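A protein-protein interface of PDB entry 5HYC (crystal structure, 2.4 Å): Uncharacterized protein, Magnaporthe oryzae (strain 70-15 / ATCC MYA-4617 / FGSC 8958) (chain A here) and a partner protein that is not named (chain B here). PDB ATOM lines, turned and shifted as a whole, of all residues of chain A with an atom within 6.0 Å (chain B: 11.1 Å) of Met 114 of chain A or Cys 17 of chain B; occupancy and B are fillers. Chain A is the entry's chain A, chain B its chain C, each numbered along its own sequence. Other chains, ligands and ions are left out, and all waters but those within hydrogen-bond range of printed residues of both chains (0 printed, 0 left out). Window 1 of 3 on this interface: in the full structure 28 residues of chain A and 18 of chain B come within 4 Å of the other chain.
Along chain A the printed residues that touch a printed residue of chain B span positions 111 to 145.
Hydrophobic or aromatic side chains of chain B that line the printed part of chain A: Ile 14, Tyr 15 and Pro 19.
Among the printed residues, 14 pairs touch across the chains.
The backbone carbonyl oxygen of Val 145 of chain A lies within hydrogen-bond range of the backbone NH of Thr 74 of chain A, 2.9 Å away.
Of chain A, only Arg 111, Arg 112, Gly 113 and Met 114 come within 4 Å of Cys 17 of chain B.
Gly 113 of chain A touches two residues of chain B.
Of chain B, only Ile 14, Tyr 15 and Glu 16 come within 4 Å of His 115 of chain A.
Of chain B, only Ile 14 and Tyr 15 come within 4 Å of Ser 116 of chain A.
Of the printed residues of chain B, Val 145 of chain A touches Tyr 15.
Of the printed residues of chain A, Ser 20 of chain B touches Arg 111.
Pro 18 of chain B touches none of the printed residues of chain A.
The nearest residue of chain B that does not touch Met 114 of chain A is Tyr 15 of chain B (4.04 Å).
Cys 17 of chain B touches Arg 111 of chain A.
O of Arg 111 of chain A touches CA of Pro 19 of chain B, at 3.4 Å.
Cys 17 of chain B touches Gly 113 of chain A (O to CA, 3.2 Å).
Pro 19 of chain B touches Gly 113 of chain A.
O of Met 114 of chain A touches CA of Glu 16 of chain B, 3.8 Å away.
His 115 of chain A touches Ile 14 of chain B.
Tyr 15 of chain B touches His 115 of chain A.
His 115 of chain A touches Glu 16 of chain B.
Ser 116 of chain A touches Ile 14 of chain B.
Tyr 15 of chain B touches Val 145 of chain A.
The backbone carbonyl oxygen of Arg 111 of chain A is in hydrogen-bond range of the backbone NH of Ser 20 of chain B (2.8 Å).
O of Arg 112 of chain A is in hydrogen-bond range of SG of Cys 17 of chain B, 3.5 Å away.
The backbone NH (N) of Cys 17 of chain B sits at hydrogen-bond distance from the backbone carbonyl oxygen (O) of Met 114 of chain A (2.9 Å).
O of Ser 116 of chain A sits at hydrogen-bond distance from N of Tyr 15 of chain B (2.5 Å).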
ATOM      1  N   THR A  74      -3.298 -35.781 -14.816  1.00  0.00           N
ATOM      2  CA  THR A  74      -4.740 -35.925 -14.677  1.00  0.00           C
ATOM      3  C   THR A  74      -5.400 -36.024 -16.041  1.00  0.00           C
ATOM      4  O   THR A  74      -5.110 -35.237 -16.908  1.00  0.00           O
ATOM      5  CB  THR A  74      -5.369 -34.734 -13.926  1.00  0.00           C
ATOM      6  OG1 THR A  74      -4.734 -34.565 -12.661  1.00  0.00           O
ATOM      7  CG2 THR A  74      -6.851 -34.940 -13.735  1.00  0.00           C
ATOM      8  N   VAL A  76      -9.122 -35.819 -17.877  1.00  0.00           N
ATOM      9  CA  VAL A  76     -10.496 -35.405 -17.621  1.00  0.00           C
ATOM     10  C   VAL A  76     -11.336 -35.534 -18.860  1.00  0.00           C
ATOM     11  O   VAL A  76     -11.042 -34.948 -19.882  1.00  0.00           O
ATOM     12  CB  VAL A  76     -10.571 -33.945 -17.103  1.00  0.00           C
ATOM     13  CG1 VAL A  76     -11.980 -33.613 -16.626  1.00  0.00           C
ATOM     14  CG2 VAL A  76      -9.596 -33.758 -15.951  1.00  0.00           C
ATOM     15  N   ARG A 111     -17.123 -28.514 -20.450  1.00  0.00           N
ATOM     16  CA  ARG A 111     -16.260 -28.935 -19.371  1.00  0.00           C
ATOM     17  C   ARG A 111     -16.887 -28.687 -18.024  1.00  0.00           C
ATOM     18  O   ARG A 111     -17.516 -27.661 -17.792  1.00  0.00           O
ATOM     19  CB  ARG A 111     -14.917 -28.213 -19.429  1.00  0.00           C
ATOM     20  CG  ARG A 111     -14.065 -28.587 -20.615  1.00  0.00           C
ATOM     21  CD  ARG A 111     -12.759 -27.815 -20.624  1.00  0.00           C
ATOM     22  NE  ARG A 111     -11.910 -28.263 -21.716  1.00  0.00           N
ATOM     23  CZ  ARG A 111     -11.798 -27.660 -22.898  1.00  0.00           C
ATOM     24  NH1 ARG A 111     -12.477 -26.550 -23.173  1.00  0.00           N
ATOM     25  NH2 ARG A 111     -11.001 -28.176 -23.819  1.00  0.00           N
ATOM     26  N   ARG A 112     -16.699 -29.640 -17.125  1.00  0.00           N
ATOM     27  CA  ARG A 112     -16.997 -29.422 -15.733  1.00  0.00           C
ATOM     28  C   ARG A 112     -16.024 -28.391 -15.143  1.00  0.00           C
ATOM     29  O   ARG A 112     -14.923 -28.208 -15.640  1.00  0.00           O
ATOM     30  CB  ARG A 112     -16.933 -30.744 -14.981  1.00  0.00           C
ATOM     31  CG  ARG A 112     -15.535 -31.327 -14.885  1.00  0.00           C
ATOM     32  CD  ARG A 112     -15.453 -32.417 -13.869  1.00  0.00           C
ATOM     33  NE  ARG A 112     -15.631 -33.759 -14.378  1.00  0.00           N
ATOM     34  CZ  ARG A 112     -16.010 -34.789 -13.623  1.00  0.00           C
ATOM     35  NH1 ARG A 112     -16.344 -34.603 -12.351  1.00  0.00           N
ATOM     36  NH2 ARG A 112     -16.098 -36.000 -14.153  1.00  0.00           N
ATOM     37  N   GLY A 113     -16.432 -27.705 -14.085  1.00  0.00           N
ATOM     38  CA  GLY A 113     -15.547 -26.760 -13.451  1.00  0.00           C
ATOM     39  C   GLY A 113     -14.523 -27.454 -12.582  1.00  0.00           C
ATOM     40  O   GLY A 113     -14.818 -28.461 -11.949  1.00  0.00           O
ATOM     41  N   MET A 114     -13.304 -26.939 -12.572  1.00  0.00           N
ATOM     42  CA  MET A 114     -12.339 -27.392 -11.593  1.00  0.00           C
ATOM     43  C   MET A 114     -11.253 -26.364 -11.348  1.00  0.00           C
ATOM     44  O   MET A 114     -10.985 -25.497 -12.169  1.00  0.00           O
ATOM     45  CB  MET A 114     -11.724 -28.739 -11.990  1.00  0.00           C
ATOM     46  CG  MET A 114     -11.276 -28.874 -13.413  1.00  0.00           C
ATOM     47  SD  MET A 114     -10.911 -30.601 -13.812  1.00  0.00           S
ATOM     48  CE  MET A 114      -9.434 -30.789 -12.850  1.00  0.00           C
ATOM     49  N   HIS A 115     -10.664 -26.452 -10.169  1.00  0.00           N
ATOM     50  CA  HIS A 115      -9.605 -25.560  -9.777  1.00  0.00           C
ATOM     51  C   HIS A 115      -8.583 -26.360  -9.006  1.00  0.00           C
ATOM     52  O   HIS A 115      -8.913 -27.020  -8.026  1.00  0.00           O
ATOM     53  CB  HIS A 115     -10.142 -24.416  -8.930  1.00  0.00           C
ATOM     54  CG  HIS A 115      -9.188 -23.283  -8.770  1.00  0.00           C
ATOM     55  ND1 HIS A 115      -8.098 -23.334  -7.936  1.00  0.00           N
ATOM     56  CD2 HIS A 115      -9.169 -22.046  -9.331  1.00  0.00           C
ATOM     57  CE1 HIS A 115      -7.444 -22.189  -7.989  1.00  0.00           C
ATOM     58  NE2 HIS A 115      -8.077 -21.395  -8.837  1.00  0.00           N
ATOM     59  N   SER A 116      -7.348 -26.300  -9.473  1.00  0.00           N
ATOM     60  CA  SER A 116      -6.244 -26.974  -8.841  1.00  0.00           C
ATOM     61  C   SER A 116      -5.188 -25.955  -8.476  1.00  0.00           C
ATOM     62  O   SER A 116      -4.722 -25.216  -9.323  1.00  0.00           O
ATOM     63  CB  SER A 116      -5.667 -28.042  -9.778  1.00  0.00           C
ATOM     64  OG  SER A 116      -4.854 -28.970  -9.093  1.00  0.00           O
ATOM     65  N   VAL A 145      -3.941 -32.690 -17.916  1.00  0.00           N
ATOM     66  CA  VAL A 145      -3.177 -31.686 -17.191  1.00  0.00           C
ATOM     67  C   VAL A 145      -1.961 -32.312 -16.507  1.00  0.00           C
ATOM     68  O   VAL A 145      -2.036 -33.375 -15.909  1.00  0.00           O
ATOM     69  CB  VAL A 145      -4.026 -30.957 -16.105  1.00  0.00           C
ATOM     70  CG1 VAL A 145      -3.245 -29.798 -15.544  1.00  0.00           C
ATOM     71  CG2 VAL A 145      -5.356 -30.442 -16.679  1.00  0.00           C
ATOM     72  N   THR B  13       0.156 -21.427  -6.502  1.00  0.00           N
ATOM     73  CA  THR B  13      -0.030 -21.396  -7.968  1.00  0.00           C
ATOM     74  C   THR B  13      -1.214 -22.271  -8.432  1.00  0.00           C
ATOM     75  O   THR B  13      -1.828 -22.917  -7.607  1.00  0.00           O
ATOM     76  CB  THR B  13       1.238 -21.858  -8.705  1.00  0.00           C
ATOM     77  OG1 THR B  13       1.176 -23.271  -8.920  1.00  0.00           O
ATOM     78  CG2 THR B  13       2.478 -21.528  -7.900  1.00  0.00           C
ATOM     79  N   ILE B  14      -1.490 -22.344  -9.747  1.00  0.00           N
ATOM     80  CA  ILE B  14      -2.800 -22.810 -10.254  1.00  0.00           C
ATOM     81  C   ILE B  14      -2.849 -23.740 -11.524  1.00  0.00           C
ATOM     82  O   ILE B  14      -1.924 -23.736 -12.326  1.00  0.00           O
ATOM     83  CB  ILE B  14      -3.669 -21.523 -10.529  1.00  0.00           C
ATOM     84  CG1 ILE B  14      -3.983 -20.806  -9.222  1.00  0.00           C
ATOM     85  CG2 ILE B  14      -4.972 -21.822 -11.240  1.00  0.00           C
ATOM     86  CD1 ILE B  14      -5.200 -19.934  -9.262  1.00  0.00           C
ATOM     87  N   TYR B  15      -3.899 -24.575 -11.642  1.00  0.00           N
ATOM     88  CA  TYR B  15      -4.564 -24.912 -12.932  1.00  0.00           C
ATOM     89  C   TYR B  15      -6.099 -24.686 -12.834  1.00  0.00           C
ATOM     90  O   TYR B  15      -6.715 -25.100 -11.863  1.00  0.00           O
ATOM     91  CB  TYR B  15      -4.333 -26.344 -13.366  1.00  0.00           C
ATOM     92  CG  TYR B  15      -5.388 -26.774 -14.375  1.00  0.00           C
ATOM     93  CD1 TYR B  15      -5.370 -26.277 -15.675  1.00  0.00           C
ATOM     94  CD2 TYR B  15      -6.423 -27.633 -14.023  1.00  0.00           C
ATOM     95  CE1 TYR B  15      -6.339 -26.639 -16.605  1.00  0.00           C
ATOM     96  CE2 TYR B  15      -7.402 -27.994 -14.941  1.00  0.00           C
ATOM     97  CZ  TYR B  15      -7.352 -27.497 -16.235  1.00  0.00           C
ATOM     98  OH  TYR B  15      -8.304 -27.849 -17.171  1.00  0.00           O
ATOM     99  N   GLU B  16      -6.733 -24.083 -13.842  1.00  0.00           N
ATOM    100  CA  GLU B  16      -8.102 -23.578 -13.666  1.00  0.00           C
ATOM    101  C   GLU B  16      -9.039 -23.680 -14.884  1.00  0.00           C
ATOM    102  O   GLU B  16      -8.688 -23.298 -15.988  1.00  0.00           O
ATOM    103  CB  GLU B  16      -8.025 -22.118 -13.215  1.00  0.00           C
ATOM    104  CG  GLU B  16      -9.342 -21.514 -12.795  1.00  0.00           C
ATOM    105  CD  GLU B  16      -9.936 -20.597 -13.847  1.00  0.00           C
ATOM    106  OE1 GLU B  16      -9.172 -19.857 -14.497  1.00  0.00           O
ATOM    107  OE2 GLU B  16     -11.170 -20.612 -14.019  1.00  0.00           O
ATOM    108  N   CYS B  17     -10.259 -24.152 -14.660  1.00  0.00           N
ATOM    109  CA  CYS B  17     -11.199 -24.369 -15.751  1.00  0.00           C
ATOM    110  C   CYS B  17     -12.661 -24.040 -15.391  1.00  0.00           C
ATOM    111  O   CYS B  17     -13.339 -24.825 -14.731  1.00  0.00           O
ATOM    112  CB  CYS B  17     -11.075 -25.817 -16.215  1.00  0.00           C
ATOM    113  SG  CYS B  17     -12.356 -26.386 -17.278  1.00  0.00           S
ATOM    114  N   PRO B  18     -13.160 -22.873 -15.841  1.00  0.00           N
ATOM    115  CA  PRO B  18     -14.557 -22.534 -15.531  1.00  0.00           C
ATOM    116  C   PRO B  18     -15.521 -23.491 -16.210  1.00  0.00           C
ATOM    117  O   PRO B  18     -15.226 -23.989 -17.298  1.00  0.00           O
ATOM    118  CB  PRO B  18     -14.706 -21.105 -16.065  1.00  0.00           C
ATOM    119  CG  PRO B  18     -13.645 -20.953 -17.065  1.00  0.00           C
ATOM    120  CD  PRO B  18     -12.507 -21.841 -16.661  1.00  0.00           C
ATOM    121  N   PRO B  19     -16.641 -23.793 -15.550  1.00  0.00           N
ATOM    122  CA  PRO B  19     -17.601 -24.703 -16.175  1.00  0.00           C
ATOM    123  C   PRO B  19     -18.112 -24.180 -17.516  1.00  0.00           C
ATOM    124  O   PRO B  19     -18.180 -22.989 -17.748  1.00  0.00           O
ATOM    125  CB  PRO B  19     -18.729 -24.802 -15.148  1.00  0.00           C
ATOM    126  CG  PRO B  19     -18.430 -23.816 -14.101  1.00  0.00           C
ATOM    127  CD  PRO B  19     -17.000 -23.458 -14.169  1.00  0.00           C
ATOM    128  N   SER B  20     -18.423 -25.099 -18.411  1.00  0.00           N
ATOM    129  CA  SER B  20     -18.833 -24.734 -19.742  1.00  0.00           C
ATOM    130  C   SER B  20     -19.905 -25.689 -20.180  1.00  0.00           C
ATOM    131  O   SER B  20     -19.771 -26.873 -20.005  1.00  0.00           O
ATOM    132  CB  SER B  20     -17.648 -24.761 -20.702  1.00  0.00           C
ATOM    133  OG  SER B  20     -18.047 -24.311 -21.972  1.00  0.00           O
ATOM    134  N   PRO B  21     -20.994 -25.170 -20.743  1.00  0.00           N
ATOM    135  CA  PRO B  21     -22.073 -26.108 -21.036  1.00  0.00           C
ATOM    136  C   PRO B  21     -21.729 -27.017 -22.206  1.00  0.00           C
ATOM    137  O   PRO B  21     -21.011 -26.610 -23.113  1.00  0.00           O
ATOM    138  CB  PRO B  21     -23.257 -25.182 -21.352  1.00  0.00           C
ATOM    139  CG  PRO B  21     -22.623 -23.938 -21.853  1.00  0.00           C
ATOM    140  CD  PRO B  21     -21.353 -23.780 -21.086  1.00  0.00           C
